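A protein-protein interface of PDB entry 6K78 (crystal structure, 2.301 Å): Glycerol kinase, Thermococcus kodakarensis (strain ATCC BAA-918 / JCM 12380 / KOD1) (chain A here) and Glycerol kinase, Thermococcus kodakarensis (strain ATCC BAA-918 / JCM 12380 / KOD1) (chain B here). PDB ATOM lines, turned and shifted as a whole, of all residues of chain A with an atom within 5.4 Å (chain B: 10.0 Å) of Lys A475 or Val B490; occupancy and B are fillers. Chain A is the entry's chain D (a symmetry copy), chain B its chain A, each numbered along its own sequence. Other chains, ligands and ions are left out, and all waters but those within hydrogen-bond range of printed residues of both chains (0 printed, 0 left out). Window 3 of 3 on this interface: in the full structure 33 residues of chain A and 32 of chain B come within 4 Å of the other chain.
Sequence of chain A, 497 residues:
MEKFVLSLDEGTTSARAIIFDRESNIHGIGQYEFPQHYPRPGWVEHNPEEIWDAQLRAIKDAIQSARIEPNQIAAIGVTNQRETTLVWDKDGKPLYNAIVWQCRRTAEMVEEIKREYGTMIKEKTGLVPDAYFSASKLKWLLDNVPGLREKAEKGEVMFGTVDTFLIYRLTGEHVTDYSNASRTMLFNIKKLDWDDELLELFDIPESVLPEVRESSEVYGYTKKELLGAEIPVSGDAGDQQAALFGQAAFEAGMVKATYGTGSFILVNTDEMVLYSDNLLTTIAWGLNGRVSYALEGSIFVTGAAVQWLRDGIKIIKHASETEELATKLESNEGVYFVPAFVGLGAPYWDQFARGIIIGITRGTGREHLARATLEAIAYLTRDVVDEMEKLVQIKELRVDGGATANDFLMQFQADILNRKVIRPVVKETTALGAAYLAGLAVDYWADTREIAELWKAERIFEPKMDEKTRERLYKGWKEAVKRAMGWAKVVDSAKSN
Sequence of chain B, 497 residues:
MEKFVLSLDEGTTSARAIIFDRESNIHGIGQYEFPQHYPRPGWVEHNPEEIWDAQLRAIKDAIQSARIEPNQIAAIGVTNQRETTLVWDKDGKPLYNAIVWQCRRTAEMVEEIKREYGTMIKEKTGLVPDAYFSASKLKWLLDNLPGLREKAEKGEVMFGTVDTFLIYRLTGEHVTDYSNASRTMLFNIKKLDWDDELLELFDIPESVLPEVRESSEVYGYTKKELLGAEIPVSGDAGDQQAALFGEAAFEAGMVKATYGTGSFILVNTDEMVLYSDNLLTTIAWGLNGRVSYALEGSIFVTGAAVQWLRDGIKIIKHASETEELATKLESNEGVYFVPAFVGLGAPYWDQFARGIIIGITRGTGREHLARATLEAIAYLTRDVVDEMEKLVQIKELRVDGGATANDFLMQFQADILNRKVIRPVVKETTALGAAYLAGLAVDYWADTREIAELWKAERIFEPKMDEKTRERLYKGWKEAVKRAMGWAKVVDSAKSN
Among the printed residues, pairs that only touch across the chains: Lys A475 with Val B490, Gly A476 with Trp B487, Glu A479 with Trp B487, Glu A479 with Val B490, Ala A480 with Trp B487, Arg A483 with Ala B484 and Arg A483 with Trp B487.
The guanidinium group (NH1) of Arg A483 sits at hydrogen-bond distance from the backbone carbonyl oxygen (O) of Met B485 (2.7 Å).
NH1 of Arg B483 lies within hydrogen-bond range of O of Arg A483, at 2.9 Å.
Lys A475 touches just one residue of chain B: Val B490 (3.4 Å).
Printed residues of chain A within 4 Å of Arg B483: Arg A483.
Of the printed residues of chain A, Ala B484 touches Arg A483.
Of the printed residues of chain A, Met B485 touches Arg A483 (2.7 Å).
Ala B488 touches none of the printed residues of chain A.
Of the printed residues of chain A, Val B490 touches Lys A475 and Glu A479.
O of Ala B484 lies within hydrogen-bond range of N of Arg B354.
O of Phe B352 is in hydrogen-bond range of N of Trp B487, at 2.9 Å.
Hydrophobic or aromatic side chains of chain B within 4 Å of the printed part of chain A: Trp B487 and Val B490.
Of the 12 printed residues of chain A, 5 touch a printed residue of chain B.
Printed residues of chain A that touch a printed residue of chain B: Lys A475, Gly A476, Glu A479, Ala A480 and Arg A483.
Hydrophobic or aromatic side chains of chain A that line the printed part of chain B: Ala A480.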
ATOM      1  N   ARG A 470      27.941  37.875  -1.556  1.00  0.00           N
ATOM      2  CA  ARG A 470      26.504  38.058  -1.707  1.00  0.00           C
ATOM      3  C   ARG A 470      25.785  36.720  -1.791  1.00  0.00           C
ATOM      4  O   ARG A 470      24.711  36.545  -1.199  1.00  0.00           O
ATOM      5  CB  ARG A 470      26.209  38.910  -2.940  1.00  0.00           C
ATOM      6  CG  ARG A 470      24.750  38.856  -3.371  1.00  0.00           C
ATOM      7  CD  ARG A 470      24.371  40.024  -4.277  1.00  0.00           C
ATOM      8  NE  ARG A 470      25.030  39.913  -5.560  1.00  0.00           N
ATOM      9  CZ  ARG A 470      26.145  40.544  -5.886  1.00  0.00           C
ATOM     10  NH1 ARG A 470      26.724  41.370  -5.018  1.00  0.00           N
ATOM     11  NH2 ARG A 470      26.675  40.341  -7.089  1.00  0.00           N
ATOM     12  N   GLU A 471      26.372  35.758  -2.508  1.00  0.00           N
ATOM     13  CA  GLU A 471      25.703  34.480  -2.725  1.00  0.00           C
ATOM     14  C   GLU A 471      25.754  33.610  -1.483  1.00  0.00           C
ATOM     15  O   GLU A 471      24.804  32.876  -1.194  1.00  0.00           O
ATOM     16  CB  GLU A 471      26.318  33.766  -3.924  1.00  0.00           C
ATOM     17  CG  GLU A 471      25.682  34.203  -5.255  1.00  0.00           C
ATOM     18  CD  GLU A 471      24.224  34.661  -5.100  1.00  0.00           C
ATOM     19  OE1 GLU A 471      23.352  33.815  -4.778  1.00  0.00           O
ATOM     20  OE2 GLU A 471      23.948  35.869  -5.292  1.00  0.00           O
ATOM     21  N   ARG A 472      26.848  33.685  -0.737  1.00  0.00           N
ATOM     22  CA  ARG A 472      26.926  33.012   0.550  1.00  0.00           C
ATOM     23  C   ARG A 472      25.853  33.541   1.506  1.00  0.00           C
ATOM     24  O   ARG A 472      25.008  32.782   1.989  1.00  0.00           O
ATOM     25  CB  ARG A 472      28.329  33.210   1.115  1.00  0.00           C
ATOM     26  CG  ARG A 472      28.683  32.399   2.310  1.00  0.00           C
ATOM     27  CD  ARG A 472      30.057  32.832   2.813  1.00  0.00           C
ATOM     28  NE  ARG A 472      29.971  33.733   3.965  1.00  0.00           N
ATOM     29  CZ  ARG A 472      30.602  34.903   4.070  1.00  0.00           C
ATOM     30  NH1 ARG A 472      31.378  35.335   3.080  1.00  0.00           N
ATOM     31  NH2 ARG A 472      30.448  35.644   5.169  1.00  0.00           N
ATOM     32  N   LEU A 473      25.854  34.860   1.760  1.00  0.00           N
ATOM     33  CA  LEU A 473      24.920  35.453   2.721  1.00  0.00           C
ATOM     34  C   LEU A 473      23.487  35.093   2.388  1.00  0.00           C
ATOM     35  O   LEU A 473      22.734  34.630   3.249  1.00  0.00           O
ATOM     36  CB  LEU A 473      25.070  36.972   2.749  1.00  0.00           C
ATOM     37  CG  LEU A 473      26.368  37.477   3.353  1.00  0.00           C
ATOM     38  CD1 LEU A 473      26.382  38.991   3.330  1.00  0.00           C
ATOM     39  CD2 LEU A 473      26.525  36.944   4.770  1.00  0.00           C
ATOM     40  N   TYR A 474      23.100  35.297   1.129  1.00  0.00           N
ATOM     41  CA  TYR A 474      21.761  34.958   0.680  1.00  0.00           C
ATOM     42  C   TYR A 474      21.518  33.458   0.729  1.00  0.00           C
ATOM     43  O   TYR A 474      20.367  33.024   0.824  1.00  0.00           O
ATOM     44  CB  TYR A 474      21.541  35.502  -0.737  1.00  0.00           C
ATOM     45  CG  TYR A 474      20.088  35.595  -1.148  1.00  0.00           C
ATOM     46  CD1 TYR A 474      19.132  36.157  -0.301  1.00  0.00           C
ATOM     47  CD2 TYR A 474      19.668  35.119  -2.382  1.00  0.00           C
ATOM     48  CE1 TYR A 474      17.792  36.238  -0.677  1.00  0.00           C
ATOM     49  CE2 TYR A 474      18.329  35.197  -2.772  1.00  0.00           C
ATOM     50  CZ  TYR A 474      17.397  35.765  -1.916  1.00  0.00           C
ATOM     51  OH  TYR A 474      16.074  35.844  -2.309  1.00  0.00           O
ATOM     52  N   LYS A 475      22.584  32.654   0.656  1.00  0.00           N
ATOM     53  CA  LYS A 475      22.442  31.216   0.851  1.00  0.00           C
ATOM     54  C   LYS A 475      22.123  30.906   2.306  1.00  0.00           C
ATOM     55  O   LYS A 475      21.161  30.182   2.602  1.00  0.00           O
ATOM     56  CB  LYS A 475      23.720  30.490   0.405  1.00  0.00           C
ATOM     57  CG  LYS A 475      23.983  29.122   1.070  1.00  0.00           C
ATOM     58  CD  LYS A 475      25.323  28.523   0.608  1.00  0.00           C
ATOM     59  CE  LYS A 475      26.424  28.725   1.650  1.00  0.00           C
ATOM     60  NZ  LYS A 475      27.798  28.642   1.056  1.00  0.00           N
ATOM     61  N   GLY A 476      22.929  31.445   3.227  1.00  0.00           N
ATOM     62  CA  GLY A 476      22.590  31.352   4.635  1.00  0.00           C
ATOM     63  C   GLY A 476      21.147  31.720   4.895  1.00  0.00           C
ATOM     64  O   GLY A 476      20.442  31.020   5.628  1.00  0.00           O
ATOM     65  N   TRP A 477      20.676  32.804   4.252  1.00  0.00           N
ATOM     66  CA  TRP A 477      19.298  33.249   4.444  1.00  0.00           C
ATOM     67  C   TRP A 477      18.318  32.230   3.894  1.00  0.00           C
ATOM     68  O   TRP A 477      17.238  32.035   4.461  1.00  0.00           O
ATOM     69  CB  TRP A 477      19.065  34.612   3.781  1.00  0.00           C
ATOM     70  CG  TRP A 477      17.597  34.923   3.546  1.00  0.00           C
ATOM     71  CD1 TRP A 477      16.892  34.755   2.387  1.00  0.00           C
ATOM     72  CD2 TRP A 477      16.658  35.431   4.511  1.00  0.00           C
ATOM     73  NE1 TRP A 477      15.580  35.142   2.563  1.00  0.00           N
ATOM     74  CE2 TRP A 477      15.411  35.561   3.856  1.00  0.00           C
ATOM     75  CE3 TRP A 477      16.754  35.804   5.858  1.00  0.00           C
ATOM     76  CZ2 TRP A 477      14.267  36.036   4.504  1.00  0.00           C
ATOM     77  CZ3 TRP A 477      15.607  36.283   6.502  1.00  0.00           C
ATOM     78  CH2 TRP A 477      14.382  36.389   5.819  1.00  0.00           C
ATOM     79  N   LYS A 478      18.671  31.574   2.781  1.00  0.00           N
ATOM     80  CA  LYS A 478      17.743  30.618   2.183  1.00  0.00           C
ATOM     81  C   LYS A 478      17.603  29.375   3.047  1.00  0.00           C
ATOM     82  O   LYS A 478      16.506  28.811   3.152  1.00  0.00           O
ATOM     83  CB  LYS A 478      18.195  30.258   0.765  1.00  0.00           C
ATOM     84  CG  LYS A 478      17.957  31.378  -0.230  1.00  0.00           C
ATOM     85  CD  LYS A 478      16.477  31.469  -0.581  1.00  0.00           C
ATOM     86  CE  LYS A 478      16.151  32.869  -1.055  1.00  0.00           C
ATOM     87  NZ  LYS A 478      14.968  32.946  -1.956  1.00  0.00           N
ATOM     88  N   GLU A 479      18.692  28.961   3.688  1.00  0.00           N
ATOM     89  CA  GLU A 479      18.632  27.858   4.640  1.00  0.00           C
ATOM     90  C   GLU A 479      17.798  28.232   5.869  1.00  0.00           C
ATOM     91  O   GLU A 479      16.903  27.477   6.276  1.00  0.00           O
ATOM     92  CB  GLU A 479      20.057  27.448   5.028  1.00  0.00           C
ATOM     93  CG  GLU A 479      20.344  25.936   4.973  1.00  0.00           C
ATOM     94  CD  GLU A 479      19.931  25.280   3.660  1.00  0.00           C
ATOM     95  OE1 GLU A 479      20.626  25.491   2.642  1.00  0.00           O
ATOM     96  OE2 GLU A 479      18.914  24.551   3.649  1.00  0.00           O
ATOM     97  N   ALA A 480      18.056  29.411   6.460  1.00  0.00           N
ATOM     98  CA  ALA A 480      17.266  29.849   7.611  1.00  0.00           C
ATOM     99  C   ALA A 480      15.773  29.830   7.309  1.00  0.00           C
ATOM    100  O   ALA A 480      14.970  29.372   8.129  1.00  0.00           O
ATOM    101  CB  ALA A 480      17.694  31.250   8.046  1.00  0.00           C
ATOM    102  N   ARG A 483      14.351  26.291   7.457  1.00  0.00           N
ATOM    103  CA  ARG A 483      14.187  25.768   8.809  1.00  0.00           C
ATOM    104  C   ARG A 483      13.057  26.438   9.582  1.00  0.00           C
ATOM    105  O   ARG A 483      12.688  25.949  10.653  1.00  0.00           O
ATOM    106  CB  ARG A 483      15.517  25.885   9.549  1.00  0.00           C
ATOM    107  CG  ARG A 483      16.654  25.306   8.725  1.00  0.00           C
ATOM    108  CD  ARG A 483      17.879  25.029   9.540  1.00  0.00           C
ATOM    109  NE  ARG A 483      18.932  24.376   8.761  1.00  0.00           N
ATOM    110  CZ  ARG A 483      20.026  23.837   9.295  1.00  0.00           C
ATOM    111  NH1 ARG A 483      20.205  23.853  10.615  1.00  0.00           N
ATOM    112  NH2 ARG A 483      20.939  23.270   8.524  1.00  0.00           N
ATOM    113  N   ASP B 350      26.083  16.076  16.834  1.00  0.00           N
ATOM    114  CA  ASP B 350      26.268  16.994  15.716  1.00  0.00           C
ATOM    115  C   ASP B 350      27.121  18.144  16.222  1.00  0.00           C
ATOM    116  O   ASP B 350      26.594  19.106  16.787  1.00  0.00           O
ATOM    117  CB  ASP B 350      24.917  17.480  15.199  1.00  0.00           C
ATOM    118  CG  ASP B 350      25.029  18.335  13.946  1.00  0.00           C
ATOM    119  OD1 ASP B 350      26.129  18.846  13.641  1.00  0.00           O
ATOM    120  OD2 ASP B 350      23.996  18.488  13.265  1.00  0.00           O
ATOM    121  N   PHE B 352      28.146  20.386  14.590  1.00  0.00           N
ATOM    122  CA  PHE B 352      27.835  21.516  13.728  1.00  0.00           C
ATOM    123  C   PHE B 352      26.435  22.065  13.967  1.00  0.00           C
ATOM    124  O   PHE B 352      26.009  22.991  13.263  1.00  0.00           O
ATOM    125  CB  PHE B 352      27.997  21.122  12.247  1.00  0.00           C
ATOM    126  CG  PHE B 352      29.377  20.617  11.901  1.00  0.00           C
ATOM    127  CD1 PHE B 352      30.465  21.477  11.902  1.00  0.00           C
ATOM    128  CD2 PHE B 352      29.588  19.282  11.585  1.00  0.00           C
ATOM    129  CE1 PHE B 352      31.746  21.015  11.595  1.00  0.00           C
ATOM    130  CE2 PHE B 352      30.872  18.812  11.271  1.00  0.00           C
ATOM    131  CZ  PHE B 352      31.950  19.686  11.279  1.00  0.00           C
ATOM    132  N   ALA B 353      25.698  21.520  14.926  1.00  0.00           N
ATOM    133  CA  ALA B 353      24.450  22.160  15.296  1.00  0.00           C
ATOM    134  C   ALA B 353      24.741  23.492  15.970  1.00  0.00           C
ATOM    135  O   ALA B 353      25.812  23.704  16.547  1.00  0.00           O
ATOM    136  CB  ALA B 353      23.619  21.270  16.216  1.00  0.00           C
ATOM    137  N   ARG B 354      23.783  24.403  15.860  1.00  0.00           N
ATOM    138  CA  ARG B 354      23.903  25.721  16.453  1.00  0.00           C
ATOM    139  C   ARG B 354      22.577  26.117  17.099  1.00  0.00           C
ATOM    140  O   ARG B 354      21.504  25.572  16.793  1.00  0.00           O
ATOM    141  CB  ARG B 354      24.356  26.752  15.398  1.00  0.00           C
ATOM    142  CG  ARG B 354      25.835  26.601  14.957  1.00  0.00           C
ATOM    143  CD  ARG B 354      26.771  26.646  16.161  1.00  0.00           C
ATOM    144  NE  ARG B 354      28.177  26.498  15.783  1.00  0.00           N
ATOM    145  CZ  ARG B 354      28.848  25.348  15.781  1.00  0.00           C
ATOM    146  NH1 ARG B 354      28.259  24.215  16.146  1.00  0.00           N
ATOM    147  NH2 ARG B 354      30.120  25.331  15.415  1.00  0.00           N
ATOM    148  N   ARG B 483      15.927  21.306  13.377  1.00  0.00           N
ATOM    149  CA  ARG B 483      16.182  22.524  12.621  1.00  0.00           C
ATOM    150  C   ARG B 483      17.417  23.267  13.100  1.00  0.00           C
ATOM    151  O   ARG B 483      17.724  24.336  12.565  1.00  0.00           O
ATOM    152  CB  ARG B 483      14.947  23.430  12.663  1.00  0.00           C
ATOM    153  CG  ARG B 483      13.703  22.747  12.059  1.00  0.00           C
ATOM    154  CD  ARG B 483      12.401  23.322  12.570  1.00  0.00           C
ATOM    155  NE  ARG B 483      11.247  22.589  12.054  1.00  0.00           N
ATOM    156  CZ  ARG B 483      10.252  23.129  11.351  1.00  0.00           C
ATOM    157  NH1 ARG B 483      10.249  24.428  11.066  1.00  0.00           N
ATOM    158  NH2 ARG B 483       9.240  22.376  10.942  1.00  0.00           N
ATOM    159  N   ALA B 484      18.141  22.712  14.065  1.00  0.00           N
ATOM    160  CA  ALA B 484      19.380  23.293  14.568  1.00  0.00           C
ATOM    161  C   ALA B 484      20.617  22.606  14.008  1.00  0.00           C
ATOM    162  O   ALA B 484      21.733  23.124  14.180  1.00  0.00           O
ATOM    163  CB  ALA B 484      19.411  23.227  16.113  1.00  0.00           C
ATOM    164  N   MET B 485      20.438  21.464  13.348  1.00  0.00           N
ATOM    165  CA  MET B 485      21.551  20.597  12.993  1.00  0.00           C
ATOM    166  C   MET B 485      22.284  21.092  11.752  1.00  0.00           C
ATOM    167  O   MET B 485      21.664  21.579  10.801  1.00  0.00           O
ATOM    168  CB  MET B 485      21.042  19.173  12.777  1.00  0.00           C
ATOM    169  CG  MET B 485      20.981  18.381  14.069  1.00  0.00           C
ATOM    170  SD  MET B 485      20.639  16.633  13.835  1.00  0.00           S
ATOM    171  CE  MET B 485      18.941  16.739  13.304  1.00  0.00           C
ATOM    172  N   GLY B 486      23.615  20.982  11.784  1.00  0.00           N
ATOM    173  CA  GLY B 486      24.471  21.263  10.639  1.00  0.00           C
ATOM    174  C   GLY B 486      24.671  22.724  10.285  1.00  0.00           C
ATOM    175  O   GLY B 486      25.280  23.018   9.251  1.00  0.00           O
ATOM    176  N   TRP B 487      24.209  23.650  11.126  1.00  0.00           N
ATOM    177  CA  TRP B 487      24.211  25.061  10.758  1.00  0.00           C
ATOM    178  C   TRP B 487      25.621  25.608  10.564  1.00  0.00           C
ATOM    179  O   TRP B 487      25.824  26.514   9.747  1.00  0.00           O
ATOM    180  CB  TRP B 487      23.465  25.877  11.827  1.00  0.00           C
ATOM    181  CG  TRP B 487      23.342  27.304  11.479  1.00  0.00           C
ATOM    182  CD1 TRP B 487      24.079  28.322  11.971  1.00  0.00           C
ATOM    183  CD2 TRP B 487      22.459  27.870  10.509  1.00  0.00           C
ATOM    184  NE1 TRP B 487      23.705  29.496  11.385  1.00  0.00           N
ATOM    185  CE2 TRP B 487      22.709  29.247  10.482  1.00  0.00           C
ATOM    186  CE3 TRP B 487      21.482  27.344   9.660  1.00  0.00           C
ATOM    187  CZ2 TRP B 487      22.014  30.120   9.634  1.00  0.00           C
ATOM    188  CZ3 TRP B 487      20.786  28.209   8.821  1.00  0.00           C
ATOM    189  CH2 TRP B 487      21.052  29.580   8.818  1.00  0.00           C
ATOM    190  N   ALA B 488      26.602  25.094  11.303  1.00  0.00           N
ATOM    191  CA  ALA B 488      27.933  25.687  11.231  1.00  0.00           C
ATOM    192  C   ALA B 488      28.581  25.510   9.856  1.00  0.00           C
ATOM    193  O   ALA B 488      29.519  26.253   9.530  1.00  0.00           O
ATOM    194  CB  ALA B 488      28.834  25.111  12.329  1.00  0.00           C
ATOM    195  N   LYS B 489      28.076  24.578   9.035  1.00  0.00           N
ATOM    196  CA  LYS B 489      28.614  24.355   7.701  1.00  0.00           C
ATOM    197  C   LYS B 489      27.853  25.094   6.604  1.00  0.00           C
ATOM    198  O   LYS B 489      28.390  25.256   5.501  1.00  0.00           O
ATOM    199  CB  LYS B 489      28.635  22.858   7.401  1.00  0.00           C
ATOM    200  CG  LYS B 489      29.721  22.124   8.162  1.00  0.00           C
ATOM    201  CD  LYS B 489      29.286  20.725   8.514  1.00  0.00           C
ATOM    202  CE  LYS B 489      29.212  19.804   7.300  1.00  0.00           C
ATOM    203  NZ  LYS B 489      28.918  18.388   7.700  1.00  0.00           N
ATOM    204  N   VAL B 490      26.620  25.539   6.871  1.00  0.00           N
ATOM    205  CA  VAL B 490      25.960  26.481   5.969  1.00  0.00           C
ATOM    206  C   VAL B 490      26.661  27.828   6.025  1.00  0.00           C
ATOM    207  O   VAL B 490      26.696  28.571   5.035  1.00  0.00           O
ATOM    208  CB  VAL B 490      24.472  26.602   6.330  1.00  0.00           C
ATOM    209  CG1 VAL B 490      23.755  27.590   5.410  1.00  0.00           C
ATOM    210  CG2 VAL B 490      23.818  25.236   6.288  1.00  0.00           C
ATOM    211  N   VAL B 491      27.241  28.153   7.172  1.00  0.00           N
ATOM    212  CA  VAL B 491      27.963  29.388   7.389  1.00  0.00           C
ATOM    213  C   VAL B 491      29.331  29.032   7.976  1.00  0.00           C
ATOM    214  O   VAL B 491      30.277  29.824   7.931  1.00  0.00           O
ATOM    215  CB  VAL B 491      27.170  30.346   8.321  1.00  0.00           C
ATOM    216  CG1 VAL B 491      25.700  30.481   7.861  1.00  0.00           C
ATOM    217  CG2 VAL B 491      27.241  29.867   9.776  1.00  0.00           C
